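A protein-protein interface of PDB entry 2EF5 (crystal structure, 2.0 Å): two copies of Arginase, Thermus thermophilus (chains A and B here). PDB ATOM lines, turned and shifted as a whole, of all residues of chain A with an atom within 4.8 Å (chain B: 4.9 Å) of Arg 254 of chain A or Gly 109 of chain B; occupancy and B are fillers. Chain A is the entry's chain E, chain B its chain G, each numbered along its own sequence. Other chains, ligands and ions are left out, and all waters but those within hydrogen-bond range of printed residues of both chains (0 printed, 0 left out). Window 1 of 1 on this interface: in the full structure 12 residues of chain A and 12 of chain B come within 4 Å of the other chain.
The backbone carbonyl oxygen (O) of Gly 253 of chain A is in hydrogen-bond range of the guanidinium group (NE) of Arg 110 of chain B (2.8 Å). O of Gly 253 of chain A sits close to O of Gly 109 of chain B, at 3.4 Å.
O of Leu 204 of chain A lies within hydrogen-bond range of NH2 of Arg 254 of chain A, at 2.9 Å. The backbone carbonyl oxygen (O) of Leu 207 of chain A lies within hydrogen-bond range of the guanidinium group (NH1) of Arg 254 of chain A, 2.6 Å away. NH1 of Arg 254 of chain A lies within hydrogen-bond range of O of Leu 210 of chain A. The backbone carbonyl oxygen (O) of Arg 254 of chain A lies within hydrogen-bond range of the backbone NH (N) of Leu 212 of chain A (2.8 Å). O of Leu 249 of chain A lies within hydrogen-bond range of OG of Ser 252 of chain A (2.7 Å). The backbone NH (N) of Arg 254 of chain A lies within hydrogen-bond range of the side-chain hydroxyl (OG) of Ser 252 of chain A, at 3.1 Å.
O of Ser 252 of chain A touches O of Gly 109 of chain B (3.8 Å). Arg 254 of chain A touches Gly 109 of chain B (CG to O, 3.0 Å).
Arg 254 of chain A touches just one residue of chain B: Gly 109 (3.0 Å). Gly 109 of chain B touches just these residues of chain A: Ser 252, Gly 253 and Arg 254. Of the printed residues of chain B, Ser 252 of chain A touches Gly 109. Of the printed residues of chain B, Gly 253 of chain A touches Gly 109 and Arg 110. Of the printed residues of chain A, Arg 110 of chain B touches Gly 253. Arg 111 of chain B touches none of the printed residues of chain A. Gly 209 of chain A touches none of the printed residues of chain B. The nearest printed residue of chain A that does not touch Gly 109 of chain B is Val 255 of chain A (6.2 Å). The nearest printed residue of chain A that does not touch Arg 110 of chain B is Arg 254 of chain A (5.0 Å).
Of the 6 printed residues of chain B, 2 touch a printed residue of chain A. Among the printed residues, 4 pairs touch across the chains. Among the printed residues, no Asp or Glu carboxylate lies within 4 Å of a Lys or Arg side-chain nitrogen of the other chain.
No position is printed for both chains. Of the 4 pairs that touch across the chains among the printed residues, none has its exchanged pair printed and touching as well.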
ATOM      1  N   LEU A 204      15.384  20.863  11.515  1.00  0.00           N
ATOM      2  CA  LEU A 204      15.490  22.007  10.618  1.00  0.00           C
ATOM      3  C   LEU A 204      14.125  22.513  10.139  1.00  0.00           C
ATOM      4  O   LEU A 204      13.931  23.711   9.916  1.00  0.00           O
ATOM      5  CB  LEU A 204      16.362  21.636   9.417  1.00  0.00           C
ATOM      6  CG  LEU A 204      17.839  21.372   9.736  1.00  0.00           C
ATOM      7  CD1 LEU A 204      18.540  20.839   8.494  1.00  0.00           C
ATOM      8  CD2 LEU A 204      18.508  22.665  10.224  1.00  0.00           C
ATOM      9  N   LEU A 207      12.362  24.324  12.990  1.00  0.00           N
ATOM     10  CA  LEU A 207      13.016  25.618  13.232  1.00  0.00           C
ATOM     11  C   LEU A 207      13.395  26.293  11.925  1.00  0.00           C
ATOM     12  O   LEU A 207      14.365  27.051  11.829  1.00  0.00           O
ATOM     13  CB  LEU A 207      14.281  25.416  14.064  1.00  0.00           C
ATOM     14  CG  LEU A 207      14.133  24.646  15.377  1.00  0.00           C
ATOM     15  CD1 LEU A 207      15.500  24.516  16.019  1.00  0.00           C
ATOM     16  CD2 LEU A 207      13.177  25.375  16.310  1.00  0.00           C
ATOM     17  N   GLN A 208      12.597  26.008  10.912  1.00  0.00           N
ATOM     18  CA  GLN A 208      12.824  26.532   9.591  1.00  0.00           C
ATOM     19  C   GLN A 208      12.862  28.051   9.451  1.00  0.00           C
ATOM     20  O   GLN A 208      11.950  28.754   9.853  1.00  0.00           O
ATOM     21  CB  GLN A 208      11.768  25.971   8.678  1.00  0.00           C
ATOM     22  CG  GLN A 208      10.427  26.503   9.020  1.00  0.00           C
ATOM     23  CD  GLN A 208       9.433  26.028   8.046  1.00  0.00           C
ATOM     24  OE1 GLN A 208       9.694  26.049   6.843  1.00  0.00           O
ATOM     25  NE2 GLN A 208       8.279  25.576   8.531  1.00  0.00           N
ATOM     26  N   GLY A 209      13.931  28.536   8.833  1.00  0.00           N
ATOM     27  CA  GLY A 209      14.102  29.962   8.614  1.00  0.00           C
ATOM     28  C   GLY A 209      14.721  30.741   9.752  1.00  0.00           C
ATOM     29  O   GLY A 209      14.910  31.936   9.651  1.00  0.00           O
ATOM     30  N   LEU A 210      15.030  30.047  10.837  1.00  0.00           N
ATOM     31  CA  LEU A 210      15.639  30.673  12.005  1.00  0.00           C
ATOM     32  C   LEU A 210      17.125  30.421  12.131  1.00  0.00           C
ATOM     33  O   LEU A 210      17.633  29.377  11.727  1.00  0.00           O
ATOM     34  CB  LEU A 210      14.994  30.197  13.323  1.00  0.00           C
ATOM     35  CG  LEU A 210      13.537  30.516  13.660  1.00  0.00           C
ATOM     36  CD1 LEU A 210      13.144  29.787  14.941  1.00  0.00           C
ATOM     37  CD2 LEU A 210      13.328  32.031  13.768  1.00  0.00           C
ATOM     38  N   PRO A 211      17.856  31.411  12.664  1.00  0.00           N
ATOM     39  CA  PRO A 211      19.285  31.147  12.810  1.00  0.00           C
ATOM     40  C   PRO A 211      19.312  30.087  13.918  1.00  0.00           C
ATOM     41  O   PRO A 211      18.378  30.010  14.723  1.00  0.00           O
ATOM     42  CB  PRO A 211      19.852  32.503  13.246  1.00  0.00           C
ATOM     43  CG  PRO A 211      18.667  33.222  13.864  1.00  0.00           C
ATOM     44  CD  PRO A 211      17.525  32.817  12.974  1.00  0.00           C
ATOM     45  N   LEU A 212      20.352  29.268  13.980  1.00  0.00           N
ATOM     46  CA  LEU A 212      20.375  28.230  15.003  1.00  0.00           C
ATOM     47  C   LEU A 212      21.542  28.243  15.974  1.00  0.00           C
ATOM     48  O   LEU A 212      22.696  28.385  15.577  1.00  0.00           O
ATOM     49  CB  LEU A 212      20.321  26.851  14.345  1.00  0.00           C
ATOM     50  CG  LEU A 212      19.146  26.594  13.402  1.00  0.00           C
ATOM     51  CD1 LEU A 212      19.372  25.290  12.656  1.00  0.00           C
ATOM     52  CD2 LEU A 212      17.852  26.558  14.184  1.00  0.00           C
ATOM     53  N   LEU A 249      23.042  19.652  10.191  1.00  0.00           N
ATOM     54  CA  LEU A 249      22.775  20.987  10.704  1.00  0.00           C
ATOM     55  C   LEU A 249      23.676  21.974   9.961  1.00  0.00           C
ATOM     56  O   LEU A 249      23.243  23.055   9.578  1.00  0.00           O
ATOM     57  CB  LEU A 249      23.046  21.053  12.217  1.00  0.00           C
ATOM     58  CG  LEU A 249      22.040  20.301  13.107  1.00  0.00           C
ATOM     59  CD1 LEU A 249      22.422  20.449  14.574  1.00  0.00           C
ATOM     60  CD2 LEU A 249      20.638  20.850  12.884  1.00  0.00           C
ATOM     61  N   SER A 252      22.528  23.179   6.485  1.00  0.00           N
ATOM     62  CA  SER A 252      21.464  24.178   6.452  1.00  0.00           C
ATOM     63  C   SER A 252      22.060  25.575   6.277  1.00  0.00           C
ATOM     64  O   SER A 252      21.438  26.457   5.687  1.00  0.00           O
ATOM     65  CB  SER A 252      20.637  24.129   7.741  1.00  0.00           C
ATOM     66  OG  SER A 252      21.328  24.753   8.816  1.00  0.00           O
ATOM     67  N   GLY A 253      23.273  25.763   6.785  1.00  0.00           N
ATOM     68  CA  GLY A 253      23.921  27.058   6.691  1.00  0.00           C
ATOM     69  C   GLY A 253      23.353  28.056   7.691  1.00  0.00           C
ATOM     70  O   GLY A 253      23.742  29.221   7.692  1.00  0.00           O
ATOM     71  N   ARG A 254      22.444  27.602   8.553  1.00  0.00           N
ATOM     72  CA  ARG A 254      21.817  28.481   9.538  1.00  0.00           C
ATOM     73  C   ARG A 254      22.423  28.476  10.944  1.00  0.00           C
ATOM     74  O   ARG A 254      22.028  29.281  11.799  1.00  0.00           O
ATOM     75  CB  ARG A 254      20.319  28.163   9.632  1.00  0.00           C
ATOM     76  CG  ARG A 254      19.549  28.485   8.352  1.00  0.00           C
ATOM     77  CD  ARG A 254      18.053  28.461   8.568  1.00  0.00           C
ATOM     78  NE  ARG A 254      17.462  27.131   8.417  1.00  0.00           N
ATOM     79  CZ  ARG A 254      16.781  26.504   9.371  1.00  0.00           C
ATOM     80  NH1 ARG A 254      16.609  27.076  10.557  1.00  0.00           N
ATOM     81  NH2 ARG A 254      16.244  25.314   9.127  1.00  0.00           N
ATOM     82  N   VAL A 255      23.375  27.585  11.200  1.00  0.00           N
ATOM     83  CA  VAL A 255      23.985  27.533  12.524  1.00  0.00           C
ATOM     84  C   VAL A 255      24.817  28.792  12.764  1.00  0.00           C
ATOM     85  O   VAL A 255      25.705  29.109  11.985  1.00  0.00           O
ATOM     86  CB  VAL A 255      24.848  26.274  12.676  1.00  0.00           C
ATOM     87  CG1 VAL A 255      25.504  26.260  14.045  1.00  0.00           C
ATOM     88  CG2 VAL A 255      23.968  25.028  12.500  1.00  0.00           C
ATOM     89  N   GLN A 256      24.536  29.493  13.858  1.00  0.00           N
ATOM     90  CA  GLN A 256      25.213  30.753  14.145  1.00  0.00           C
ATOM     91  C   GLN A 256      26.052  30.810  15.401  1.00  0.00           C
ATOM     92  O   GLN A 256      26.821  31.747  15.576  1.00  0.00           O
ATOM     93  CB  GLN A 256      24.177  31.869  14.228  1.00  0.00           C
ATOM     94  CG  GLN A 256      23.169  31.654  15.343  1.00  0.00           C
ATOM     95  CD  GLN A 256      22.842  32.936  16.078  1.00  0.00           C
ATOM     96  OE1 GLN A 256      22.360  33.896  15.484  1.00  0.00           O
ATOM     97  NE2 GLN A 256      23.105  32.954  17.380  1.00  0.00           N
ATOM     98  N   ALA B 104      13.411  34.111   0.314  1.00  0.00           N
ATOM     99  CA  ALA B 104      13.754  32.831   0.913  1.00  0.00           C
ATOM    100  C   ALA B 104      14.751  32.114   0.014  1.00  0.00           C
ATOM    101  O   ALA B 104      15.740  31.569   0.492  1.00  0.00           O
ATOM    102  CB  ALA B 104      12.498  31.980   1.105  1.00  0.00           C
ATOM    103  N   ALA B 107      18.206  33.999  -0.250  1.00  0.00           N
ATOM    104  CA  ALA B 107      18.921  33.995   1.022  1.00  0.00           C
ATOM    105  C   ALA B 107      19.905  32.829   1.117  1.00  0.00           C
ATOM    106  O   ALA B 107      20.946  32.932   1.775  1.00  0.00           O
ATOM    107  CB  ALA B 107      17.930  33.936   2.170  1.00  0.00           C
ATOM    108  N   ARG B 108      19.574  31.724   0.455  1.00  0.00           N
ATOM    109  CA  ARG B 108      20.428  30.541   0.453  1.00  0.00           C
ATOM    110  C   ARG B 108      20.722  30.021   1.852  1.00  0.00           C
ATOM    111  O   ARG B 108      21.840  29.607   2.147  1.00  0.00           O
ATOM    112  CB  ARG B 108      21.751  30.838  -0.254  1.00  0.00           C
ATOM    113  CG  ARG B 108      21.600  31.132  -1.726  1.00  0.00           C
ATOM    114  CD  ARG B 108      22.943  31.098  -2.442  1.00  0.00           C
ATOM    115  NE  ARG B 108      22.734  30.983  -3.880  1.00  0.00           N
ATOM    116  CZ  ARG B 108      22.084  29.972  -4.446  1.00  0.00           C
ATOM    117  NH1 ARG B 108      21.597  28.993  -3.694  1.00  0.00           N
ATOM    118  NH2 ARG B 108      21.892  29.954  -5.754  1.00  0.00           N
ATOM    119  N   GLY B 109      19.713  30.047   2.716  1.00  0.00           N
ATOM    120  CA  GLY B 109      19.896  29.556   4.069  1.00  0.00           C
ATOM    121  C   GLY B 109      20.738  30.431   4.980  1.00  0.00           C
ATOM    122  O   GLY B 109      20.860  30.141   6.168  1.00  0.00           O
ATOM    123  N   ARG B 110      21.324  31.499   4.449  1.00  0.00           N
ATOM    124  CA  ARG B 110      22.135  32.378   5.282  1.00  0.00           C
ATOM    125  C   ARG B 110      21.364  33.623   5.707  1.00  0.00           C
ATOM    126  O   ARG B 110      20.313  33.937   5.149  1.00  0.00           O
ATOM    127  CB  ARG B 110      23.415  32.780   4.549  1.00  0.00           C
ATOM    128  CG  ARG B 110      24.372  33.624   5.387  1.00  0.00           C
ATOM    129  CD  ARG B 110      24.523  33.080   6.813  1.00  0.00           C
ATOM    130  NE  ARG B 110      24.918  31.671   6.839  1.00  0.00           N
ATOM    131  CZ  ARG B 110      26.143  31.231   6.576  1.00  0.00           C
ATOM    132  NH1 ARG B 110      27.105  32.089   6.267  1.00  0.00           N
ATOM    133  NH2 ARG B 110      26.405  29.931   6.617  1.00  0.00           N
ATOM    134  N   ARG B 111      21.896  34.316   6.709  1.00  0.00           N
ATOM    135  CA  ARG B 111      21.282  35.526   7.242  1.00  0.00           C
ATOM    136  C   ARG B 111      21.447  36.676   6.251  1.00  0.00           C
ATOM    137  O   ARG B 111      22.566  37.025   5.871  1.00  0.00           O
ATOM    138  CB  ARG B 111      21.940  35.887   8.583  1.00  0.00           C
ATOM    139  CG  ARG B 111      21.316  37.069   9.306  1.00  0.00           C
ATOM    140  CD  ARG B 111      22.126  37.476  10.544  1.00  0.00           C
ATOM    141  NE  ARG B 111      21.537  38.635  11.219  1.00  0.00           N
ATOM    142  CZ  ARG B 111      22.136  39.334  12.182  1.00  0.00           C
ATOM    143  NH1 ARG B 111      23.358  39.005  12.601  1.00  0.00           N
ATOM    144  NH2 ARG B 111      21.509  40.362  12.732  1.00  0.00           N
